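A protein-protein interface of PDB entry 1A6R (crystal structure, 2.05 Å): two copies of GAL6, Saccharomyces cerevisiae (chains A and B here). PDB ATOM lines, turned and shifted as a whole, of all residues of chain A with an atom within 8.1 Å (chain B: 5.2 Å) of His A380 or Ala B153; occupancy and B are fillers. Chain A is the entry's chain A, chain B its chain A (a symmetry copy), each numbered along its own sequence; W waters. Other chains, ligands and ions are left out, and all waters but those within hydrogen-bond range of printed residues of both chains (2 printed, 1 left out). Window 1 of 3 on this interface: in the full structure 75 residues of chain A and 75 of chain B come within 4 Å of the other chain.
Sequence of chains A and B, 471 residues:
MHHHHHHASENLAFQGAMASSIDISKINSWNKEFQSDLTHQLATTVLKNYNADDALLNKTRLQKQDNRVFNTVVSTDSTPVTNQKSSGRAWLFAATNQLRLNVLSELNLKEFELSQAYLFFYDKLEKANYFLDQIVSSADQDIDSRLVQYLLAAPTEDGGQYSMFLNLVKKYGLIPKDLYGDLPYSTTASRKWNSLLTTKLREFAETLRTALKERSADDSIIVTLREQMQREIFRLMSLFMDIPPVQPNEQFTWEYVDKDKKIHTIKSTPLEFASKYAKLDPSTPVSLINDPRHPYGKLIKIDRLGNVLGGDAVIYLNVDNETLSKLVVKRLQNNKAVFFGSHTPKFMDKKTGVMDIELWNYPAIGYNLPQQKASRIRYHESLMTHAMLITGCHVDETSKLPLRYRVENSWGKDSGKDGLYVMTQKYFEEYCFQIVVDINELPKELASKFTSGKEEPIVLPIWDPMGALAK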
ATOM      1  N   ARG A 146      22.182  19.533 -36.376  1.00  0.00           N
ATOM      2  CA  ARG A 146      21.860  18.762 -35.199  1.00  0.00           C
ATOM      3  C   ARG A 146      22.935  17.738 -34.851  1.00  0.00           C
ATOM      4  O   ARG A 146      23.239  17.524 -33.684  1.00  0.00           O
ATOM      5  CB  ARG A 146      20.510  18.063 -35.389  1.00  0.00           C
ATOM      6  CG  ARG A 146      19.824  17.666 -34.104  1.00  0.00           C
ATOM      7  CD  ARG A 146      18.450  17.144 -34.437  1.00  0.00           C
ATOM      8  NE  ARG A 146      17.669  16.786 -33.259  1.00  0.00           N
ATOM      9  CZ  ARG A 146      16.513  16.133 -33.316  1.00  0.00           C
ATOM     10  NH1 ARG A 146      16.008  15.784 -34.488  1.00  0.00           N
ATOM     11  NH2 ARG A 146      15.886  15.767 -32.213  1.00  0.00           N
ATOM     12  N   HIS A 343      15.171   4.639 -15.594  1.00  0.00           N
ATOM     13  CA  HIS A 343      15.044   6.066 -15.463  1.00  0.00           C
ATOM     14  C   HIS A 343      15.188   6.535 -13.998  1.00  0.00           C
ATOM     15  O   HIS A 343      14.195   6.884 -13.342  1.00  0.00           O
ATOM     16  CB  HIS A 343      13.707   6.557 -16.043  1.00  0.00           C
ATOM     17  CG  HIS A 343      13.634   8.047 -16.155  1.00  0.00           C
ATOM     18  ND1 HIS A 343      12.553   8.704 -16.699  1.00  0.00           N
ATOM     19  CD2 HIS A 343      14.501   9.010 -15.769  1.00  0.00           C
ATOM     20  CE1 HIS A 343      12.757  10.008 -16.637  1.00  0.00           C
ATOM     21  NE2 HIS A 343      13.932  10.223 -16.075  1.00  0.00           N
ATOM     22  N   GLN A 371      -0.241   9.514 -19.444  1.00  0.00           N
ATOM     23  CA  GLN A 371       0.664   9.253 -20.565  1.00  0.00           C
ATOM     24  C   GLN A 371       1.337   7.898 -20.421  1.00  0.00           C
ATOM     25  O   GLN A 371       1.877   7.563 -19.361  1.00  0.00           O
ATOM     26  CB  GLN A 371       1.684  10.378 -20.696  1.00  0.00           C
ATOM     27  CG  GLN A 371       2.313  10.490 -22.071  1.00  0.00           C
ATOM     28  CD  GLN A 371       3.128  11.750 -22.203  1.00  0.00           C
ATOM     29  OE1 GLN A 371       3.934  12.064 -21.328  1.00  0.00           O
ATOM     30  NE2 GLN A 371       2.901  12.505 -23.272  1.00  0.00           N
ATOM     31  N   ALA A 374       5.322   4.445 -24.284  1.00  0.00           N
ATOM     32  CA  ALA A 374       5.783   4.844 -25.604  1.00  0.00           C
ATOM     33  C   ALA A 374       5.738   6.330 -25.770  1.00  0.00           C
ATOM     34  O   ALA A 374       6.643   6.942 -26.355  1.00  0.00           O
ATOM     35  CB  ALA A 374       4.929   4.185 -26.678  1.00  0.00           C
ATOM     36  N   SER A 375       4.663   6.930 -25.285  1.00  0.00           N
ATOM     37  CA  SER A 375       4.476   8.361 -25.396  1.00  0.00           C
ATOM     38  C   SER A 375       5.418   9.140 -24.499  1.00  0.00           C
ATOM     39  O   SER A 375       5.858  10.229 -24.874  1.00  0.00           O
ATOM     40  CB  SER A 375       3.020   8.719 -25.086  1.00  0.00           C
ATOM     41  OG  SER A 375       2.152   8.172 -26.066  1.00  0.00           O
ATOM     42  N   ARG A 376       5.700   8.600 -23.308  1.00  0.00           N
ATOM     43  CA  ARG A 376       6.626   9.249 -22.366  1.00  0.00           C
ATOM     44  C   ARG A 376       8.008   9.354 -23.010  1.00  0.00           C
ATOM     45  O   ARG A 376       8.717  10.342 -22.832  1.00  0.00           O
ATOM     46  CB  ARG A 376       6.729   8.431 -21.083  1.00  0.00           C
ATOM     47  CG  ARG A 376       5.497   8.510 -20.190  1.00  0.00           C
ATOM     48  CD  ARG A 376       5.844   8.073 -18.749  1.00  0.00           C
ATOM     49  NE  ARG A 376       6.223   6.661 -18.597  1.00  0.00           N
ATOM     50  CZ  ARG A 376       5.356   5.659 -18.444  1.00  0.00           C
ATOM     51  NH1 ARG A 376       4.042   5.884 -18.446  1.00  0.00           N
ATOM     52  NH2 ARG A 376       5.806   4.439 -18.209  1.00  0.00           N
ATOM     53  N   ILE A 377       8.395   8.295 -23.720  1.00  0.00           N
ATOM     54  CA  ILE A 377       9.675   8.244 -24.456  1.00  0.00           C
ATOM     55  C   ILE A 377       9.647   9.272 -25.609  1.00  0.00           C
ATOM     56  O   ILE A 377      10.552  10.087 -25.741  1.00  0.00           O
ATOM     57  CB  ILE A 377       9.926   6.838 -25.052  1.00  0.00           C
ATOM     58  CG1 ILE A 377       9.964   5.773 -23.956  1.00  0.00           C
ATOM     59  CG2 ILE A 377      11.247   6.823 -25.831  1.00  0.00           C
ATOM     60  CD1 ILE A 377       9.974   4.341 -24.501  1.00  0.00           C
ATOM     61  N   ARG A 378       8.600   9.235 -26.434  1.00  0.00           N
ATOM     62  CA  ARG A 378       8.449  10.163 -27.555  1.00  0.00           C
ATOM     63  C   ARG A 378       8.464  11.593 -27.132  1.00  0.00           C
ATOM     64  O   ARG A 378       8.959  12.449 -27.861  1.00  0.00           O
ATOM     65  CB  ARG A 378       7.092  10.021 -28.228  1.00  0.00           C
ATOM     66  CG  ARG A 378       6.939   8.874 -29.088  1.00  0.00           C
ATOM     67  CD  ARG A 378       5.832   9.132 -30.082  1.00  0.00           C
ATOM     68  NE  ARG A 378       5.632   7.883 -30.781  1.00  0.00           N
ATOM     69  CZ  ARG A 378       4.839   6.919 -30.331  1.00  0.00           C
ATOM     70  NH1 ARG A 378       4.154   7.103 -29.202  1.00  0.00           N
ATOM     71  NH2 ARG A 378       4.815   5.737 -30.946  1.00  0.00           N
ATOM     72  N   TYR A 379       7.740  11.855 -26.044  1.00  0.00           N
ATOM     73  CA  TYR A 379       7.578  13.204 -25.523  1.00  0.00           C
ATOM     74  C   TYR A 379       8.636  13.774 -24.582  1.00  0.00           C
ATOM     75  O   TYR A 379       8.371  14.724 -23.859  1.00  0.00           O
ATOM     76  CB  TYR A 379       6.150  13.409 -24.987  1.00  0.00           C
ATOM     77  CG  TYR A 379       5.150  13.605 -26.116  1.00  0.00           C
ATOM     78  CD1 TYR A 379       4.681  12.518 -26.856  1.00  0.00           C
ATOM     79  CD2 TYR A 379       4.756  14.881 -26.502  1.00  0.00           C
ATOM     80  CE1 TYR A 379       3.850  12.706 -27.975  1.00  0.00           C
ATOM     81  CE2 TYR A 379       3.924  15.083 -27.606  1.00  0.00           C
ATOM     82  CZ  TYR A 379       3.479  14.000 -28.347  1.00  0.00           C
ATOM     83  OH  TYR A 379       2.686  14.230 -29.463  1.00  0.00           O
ATOM     84  N   HIS A 380       9.832  13.195 -24.603  1.00  0.00           N
ATOM     85  CA  HIS A 380      10.950  13.723 -23.817  1.00  0.00           C
ATOM     86  C   HIS A 380      10.780  13.591 -22.304  1.00  0.00           C
ATOM     87  O   HIS A 380      11.472  14.259 -21.538  1.00  0.00           O
ATOM     88  CB  HIS A 380      11.093  15.202 -24.191  1.00  0.00           C
ATOM     89  CG  HIS A 380      12.484  15.732 -24.125  1.00  0.00           C
ATOM     90  ND1 HIS A 380      13.269  15.636 -22.998  1.00  0.00           N
ATOM     91  CD2 HIS A 380      13.215  16.417 -25.039  1.00  0.00           C
ATOM     92  CE1 HIS A 380      14.420  16.242 -23.217  1.00  0.00           C
ATOM     93  NE2 HIS A 380      14.413  16.722 -24.449  1.00  0.00           N
ATOM     94  N   GLU A 381       9.904  12.701 -21.866  1.00  0.00           N
ATOM     95  CA  GLU A 381       9.664  12.565 -20.452  1.00  0.00           C
ATOM     96  C   GLU A 381      10.451  11.444 -19.790  1.00  0.00           C
ATOM     97  O   GLU A 381      10.804  11.552 -18.609  1.00  0.00           O
ATOM     98  CB  GLU A 381       8.155  12.396 -20.199  1.00  0.00           C
ATOM     99  CG  GLU A 381       7.771  12.022 -18.746  1.00  0.00           C
ATOM    100  CD  GLU A 381       8.106  13.111 -17.715  1.00  0.00           C
ATOM    101  OE1 GLU A 381       8.265  14.305 -18.079  1.00  0.00           O
ATOM    102  OE2 GLU A 381       8.201  12.758 -16.524  1.00  0.00           O
ATOM    103  N   SER A 382      10.767  10.390 -20.533  1.00  0.00           N
ATOM    104  CA  SER A 382      11.458   9.282 -19.917  1.00  0.00           C
ATOM    105  C   SER A 382      12.411   8.575 -20.873  1.00  0.00           C
ATOM    106  O   SER A 382      12.126   8.477 -22.063  1.00  0.00           O
ATOM    107  CB  SER A 382      10.435   8.298 -19.348  1.00  0.00           C
ATOM    108  OG  SER A 382      11.040   7.392 -18.430  1.00  0.00           O
ATOM    109  N   LEU A 383      13.518   8.064 -20.318  1.00  0.00           N
ATOM    110  CA  LEU A 383      14.598   7.383 -21.055  1.00  0.00           C
ATOM    111  C   LEU A 383      15.522   6.755 -19.995  1.00  0.00           C
ATOM    112  O   LEU A 383      15.414   7.076 -18.813  1.00  0.00           O
ATOM    113  CB  LEU A 383      15.430   8.429 -21.804  1.00  0.00           C
ATOM    114  CG  LEU A 383      16.187   9.346 -20.819  1.00  0.00           C
ATOM    115  CD1 LEU A 383      17.439   9.932 -21.404  1.00  0.00           C
ATOM    116  CD2 LEU A 383      15.286  10.438 -20.301  1.00  0.00           C
ATOM    117  N   TRP A 463      20.599  11.064 -31.419  1.00  0.00           N
ATOM    118  CA  TRP A 463      19.843  11.842 -30.430  1.00  0.00           C
ATOM    119  C   TRP A 463      18.499  11.203 -30.062  1.00  0.00           C
ATOM    120  O   TRP A 463      17.725  11.787 -29.321  1.00  0.00           O
ATOM    121  CB  TRP A 463      19.592  13.265 -30.950  1.00  0.00           C
ATOM    122  CG  TRP A 463      18.958  13.285 -32.333  1.00  0.00           C
ATOM    123  CD1 TRP A 463      17.663  12.983 -32.654  1.00  0.00           C
ATOM    124  CD2 TRP A 463      19.609  13.620 -33.562  1.00  0.00           C
ATOM    125  NE1 TRP A 463      17.470  13.114 -34.015  1.00  0.00           N
ATOM    126  CE2 TRP A 463      18.649  13.506 -34.592  1.00  0.00           C
ATOM    127  CE3 TRP A 463      20.909  14.009 -33.893  1.00  0.00           C
ATOM    128  CZ2 TRP A 463      18.949  13.772 -35.924  1.00  0.00           C
ATOM    129  CZ3 TRP A 463      21.209  14.271 -35.223  1.00  0.00           C
ATOM    130  CH2 TRP A 463      20.234  14.154 -36.221  1.00  0.00           C
ATOM    131  N   PRO A 465      15.870   9.120 -28.052  1.00  0.00           N
ATOM    132  CA  PRO A 465      15.815   8.732 -26.639  1.00  0.00           C
ATOM    133  C   PRO A 465      16.349   7.343 -26.308  1.00  0.00           C
ATOM    134  O   PRO A 465      16.905   7.119 -25.241  1.00  0.00           O
ATOM    135  CB  PRO A 465      14.328   8.882 -26.282  1.00  0.00           C
ATOM    136  CG  PRO A 465      13.621   9.204 -27.590  1.00  0.00           C
ATOM    137  CD  PRO A 465      14.664   9.876 -28.423  1.00  0.00           C
ATOM    138  N   GLN B 149      11.255  18.726 -30.082  1.00  0.00           N
ATOM    139  CA  GLN B 149      12.005  18.141 -28.966  1.00  0.00           C
ATOM    140  C   GLN B 149      12.558  19.260 -28.094  1.00  0.00           C
ATOM    141  O   GLN B 149      12.524  19.167 -26.867  1.00  0.00           O
ATOM    142  CB  GLN B 149      13.121  17.194 -29.449  1.00  0.00           C
ATOM    143  CG  GLN B 149      12.553  15.860 -29.904  1.00  0.00           C
ATOM    144  CD  GLN B 149      11.763  15.173 -28.793  1.00  0.00           C
ATOM    145  OE1 GLN B 149      12.279  14.987 -27.710  1.00  0.00           O
ATOM    146  NE2 GLN B 149      10.516  14.823 -29.049  1.00  0.00           N
ATOM    147  N   TYR B 150      12.988  20.345 -28.726  1.00  0.00           N
ATOM    148  CA  TYR B 150      13.511  21.487 -28.005  1.00  0.00           C
ATOM    149  C   TYR B 150      12.400  22.156 -27.152  1.00  0.00           C
ATOM    150  O   TYR B 150      12.688  22.683 -26.072  1.00  0.00           O
ATOM    151  CB  TYR B 150      14.121  22.494 -28.984  1.00  0.00           C
ATOM    152  CG  TYR B 150      14.865  23.612 -28.297  1.00  0.00           C
ATOM    153  CD1 TYR B 150      14.180  24.680 -27.725  1.00  0.00           C
ATOM    154  CD2 TYR B 150      16.233  23.594 -28.191  1.00  0.00           C
ATOM    155  CE1 TYR B 150      14.834  25.690 -27.069  1.00  0.00           C
ATOM    156  CE2 TYR B 150      16.911  24.624 -27.524  1.00  0.00           C
ATOM    157  CZ  TYR B 150      16.201  25.656 -26.969  1.00  0.00           C
ATOM    158  OH  TYR B 150      16.829  26.665 -26.291  1.00  0.00           O
ATOM    159  N   LEU B 151      11.153  22.163 -27.648  1.00  0.00           N
ATOM    160  CA  LEU B 151      10.021  22.738 -26.912  1.00  0.00           C
ATOM    161  C   LEU B 151       9.731  21.885 -25.693  1.00  0.00           C
ATOM    162  O   LEU B 151       9.502  22.402 -24.615  1.00  0.00           O
ATOM    163  CB  LEU B 151       8.762  22.795 -27.789  1.00  0.00           C
ATOM    164  CG  LEU B 151       8.852  23.755 -28.974  1.00  0.00           C
ATOM    165  CD1 LEU B 151       7.612  23.671 -29.847  1.00  0.00           C
ATOM    166  CD2 LEU B 151       9.056  25.168 -28.478  1.00  0.00           C
ATOM    167  N   LEU B 152       9.824  20.576 -25.867  1.00  0.00           N
ATOM    168  CA  LEU B 152       9.575  19.616 -24.809  1.00  0.00           C
ATOM    169  C   LEU B 152      10.676  19.454 -23.758  1.00  0.00           C
ATOM    170  O   LEU B 152      10.443  18.826 -22.736  1.00  0.00           O
ATOM    171  CB  LEU B 152       9.342  18.248 -25.448  1.00  0.00           C
ATOM    172  CG  LEU B 152       8.098  18.135 -26.340  1.00  0.00           C
ATOM    173  CD1 LEU B 152       8.155  16.814 -27.104  1.00  0.00           C
ATOM    174  CD2 LEU B 152       6.838  18.198 -25.474  1.00  0.00           C
ATOM    175  N   ALA B 153      11.857  20.014 -24.013  1.00  0.00           N
ATOM    176  CA  ALA B 153      13.023  19.867 -23.120  1.00  0.00           C
ATOM    177  C   ALA B 153      12.926  20.528 -21.749  1.00  0.00           C
ATOM    178  O   ALA B 153      13.089  19.856 -20.737  1.00  0.00           O
ATOM    179  CB  ALA B 153      14.304  20.312 -23.839  1.00  0.00           C
ATOM    180  N   ALA B 154      12.645  21.829 -21.725  1.00  0.00           N
ATOM    181  CA  ALA B 154      12.515  22.574 -20.474  1.00  0.00           C
ATOM    182  C   ALA B 154      11.527  23.729 -20.600  1.00  0.00           C
ATOM    183  O   ALA B 154      11.900  24.883 -20.396  1.00  0.00           O
ATOM    184  CB  ALA B 154      13.858  23.125 -20.069  1.00  0.00           C
ATOM    185  N   PRO B 155      10.245  23.438 -20.902  1.00  0.00           N
ATOM    186  CA  PRO B 155       9.216  24.485 -21.046  1.00  0.00           C
ATOM    187  C   PRO B 155       9.027  25.460 -19.863  1.00  0.00           C
ATOM    188  O   PRO B 155       8.759  26.643 -20.084  1.00  0.00           O
ATOM    189  CB  PRO B 155       7.927  23.689 -21.349  1.00  0.00           C
ATOM    190  CG  PRO B 155       8.166  22.364 -20.748  1.00  0.00           C
ATOM    191  CD  PRO B 155       9.650  22.099 -21.060  1.00  0.00           C
ATOM    192  N   THR B 198       6.320  20.060 -15.740  1.00  0.00           N
ATOM    193  CA  THR B 198       6.794  19.624 -17.034  1.00  0.00           C
ATOM    194  C   THR B 198       6.304  18.242 -17.463  1.00  0.00           C
ATOM    195  O   THR B 198       6.048  18.013 -18.642  1.00  0.00           O
ATOM    196  CB  THR B 198       8.319  19.769 -17.110  1.00  0.00           C
ATOM    197  OG1 THR B 198       8.645  21.156 -16.938  1.00  0.00           O
ATOM    198  CG2 THR B 198       8.860  19.283 -18.452  1.00  0.00           C
ATOM    199  N   ARG B 202       4.059  17.775 -20.841  1.00  0.00           N
ATOM    200  CA  ARG B 202       4.436  16.829 -21.896  1.00  0.00           C
ATOM    201  C   ARG B 202       3.248  15.954 -22.256  1.00  0.00           C
ATOM    202  O   ARG B 202       3.075  15.529 -23.410  1.00  0.00           O
ATOM    203  CB  ARG B 202       5.668  16.011 -21.489  1.00  0.00           C
ATOM    204  CG  ARG B 202       6.969  16.804 -21.663  1.00  0.00           C
ATOM    205  CD  ARG B 202       8.146  16.093 -21.005  1.00  0.00           C
ATOM    206  NE  ARG B 202       9.333  16.943 -21.036  1.00  0.00           N
ATOM    207  CZ  ARG B 202      10.320  16.878 -20.143  1.00  0.00           C
ATOM    208  NH1 ARG B 202      10.259  16.001 -19.154  1.00  0.00           N
ATOM    209  NH2 ARG B 202      11.341  17.720 -20.218  1.00  0.00           N
HETATM  210  O   HOH W   1       9.352  15.941 -15.883  1.00  0.00           O
HETATM  211  O   HOH W   2      10.964  11.529 -29.579  1.00  0.00           O
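The side-chain amide nitrogen of Gln A371 sits at hydrogen-bond distance from the backbone carbonyl oxygen of Arg B202, 3.0 Å away. NH1 of Arg B202 is in salt-bridge range of OE1 of Glu A381, at 2.8 Å. The guanidinium group (NH1) of Arg B202 sits close to the backbone carbonyl oxygen (O) of His A380 (3.2 Å). The side-chain amide nitrogen (NE2) of Gln B149 is in hydrogen-bond range of the backbone carbonyl oxygen (O) of Arg A378, at 3.1 Å.
The backbone carbonyl oxygen of Gln A371 lies within hydrogen-bond range of the guanidinium group of Arg A376. NE of Arg B202 lies within hydrogen-bond range of O of Leu B152, at 2.8 Å. The backbone carbonyl oxygen of Ala B153 lies within hydrogen-bond range of the guanidinium group of Arg B202, at 2.8 Å. N of Glu A381 sits at hydrogen-bond distance from O of Arg A376 (2.8 Å).
Among the printed residues, pairs that only touch across the chains: Tyr A379 with Leu B152 (3.9 Å), Tyr A379 with Arg B202 (3.2 Å), His A380 with Gln B149 (3.2 Å), His A380 with Leu B152 (3.7 Å) and His A380 with Ala B153 (3.6 Å).
His A380 touches just these residues of chain B: Gln B149 (3.2 Å), Leu B152 (3.7 Å), Ala B153 (3.6 Å) and Arg B202 (3.2 Å). Ala B153 touches just one residue of chain A: His A380. Of the printed residues of chain A, Arg B202 touches Gln A371, Tyr A379, His A380 and Glu A381. Of the printed residues of chain B, Arg A378 touches Gln B149 (3.1 Å). Printed residues of chain A within 4 Å of Gln B149: Arg A378 and His A380. The nearest printed residue of chain B that does not touch Gln A371 is Thr B198 (6.9 Å).
Of the 15 printed residues of chain A, 5 touch a printed residue of chain B. Among the printed residues, Asp or Glu carboxylates within 4 Å of a Lys or Arg side-chain nitrogen of the other chain: Glu A381 with Arg B202 (2.8 Å).
No position is printed for both chains.
Water W2 lies within hydrogen-bond range of the backbone carbonyl oxygen of Arg A378 (2.8 Å) and the side-chain amide nitrogen of Gln B149 (3.4 Å). Water W1 bridges the side-chain carboxylate of Glu A381 and the guanidinium group of Arg B202.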
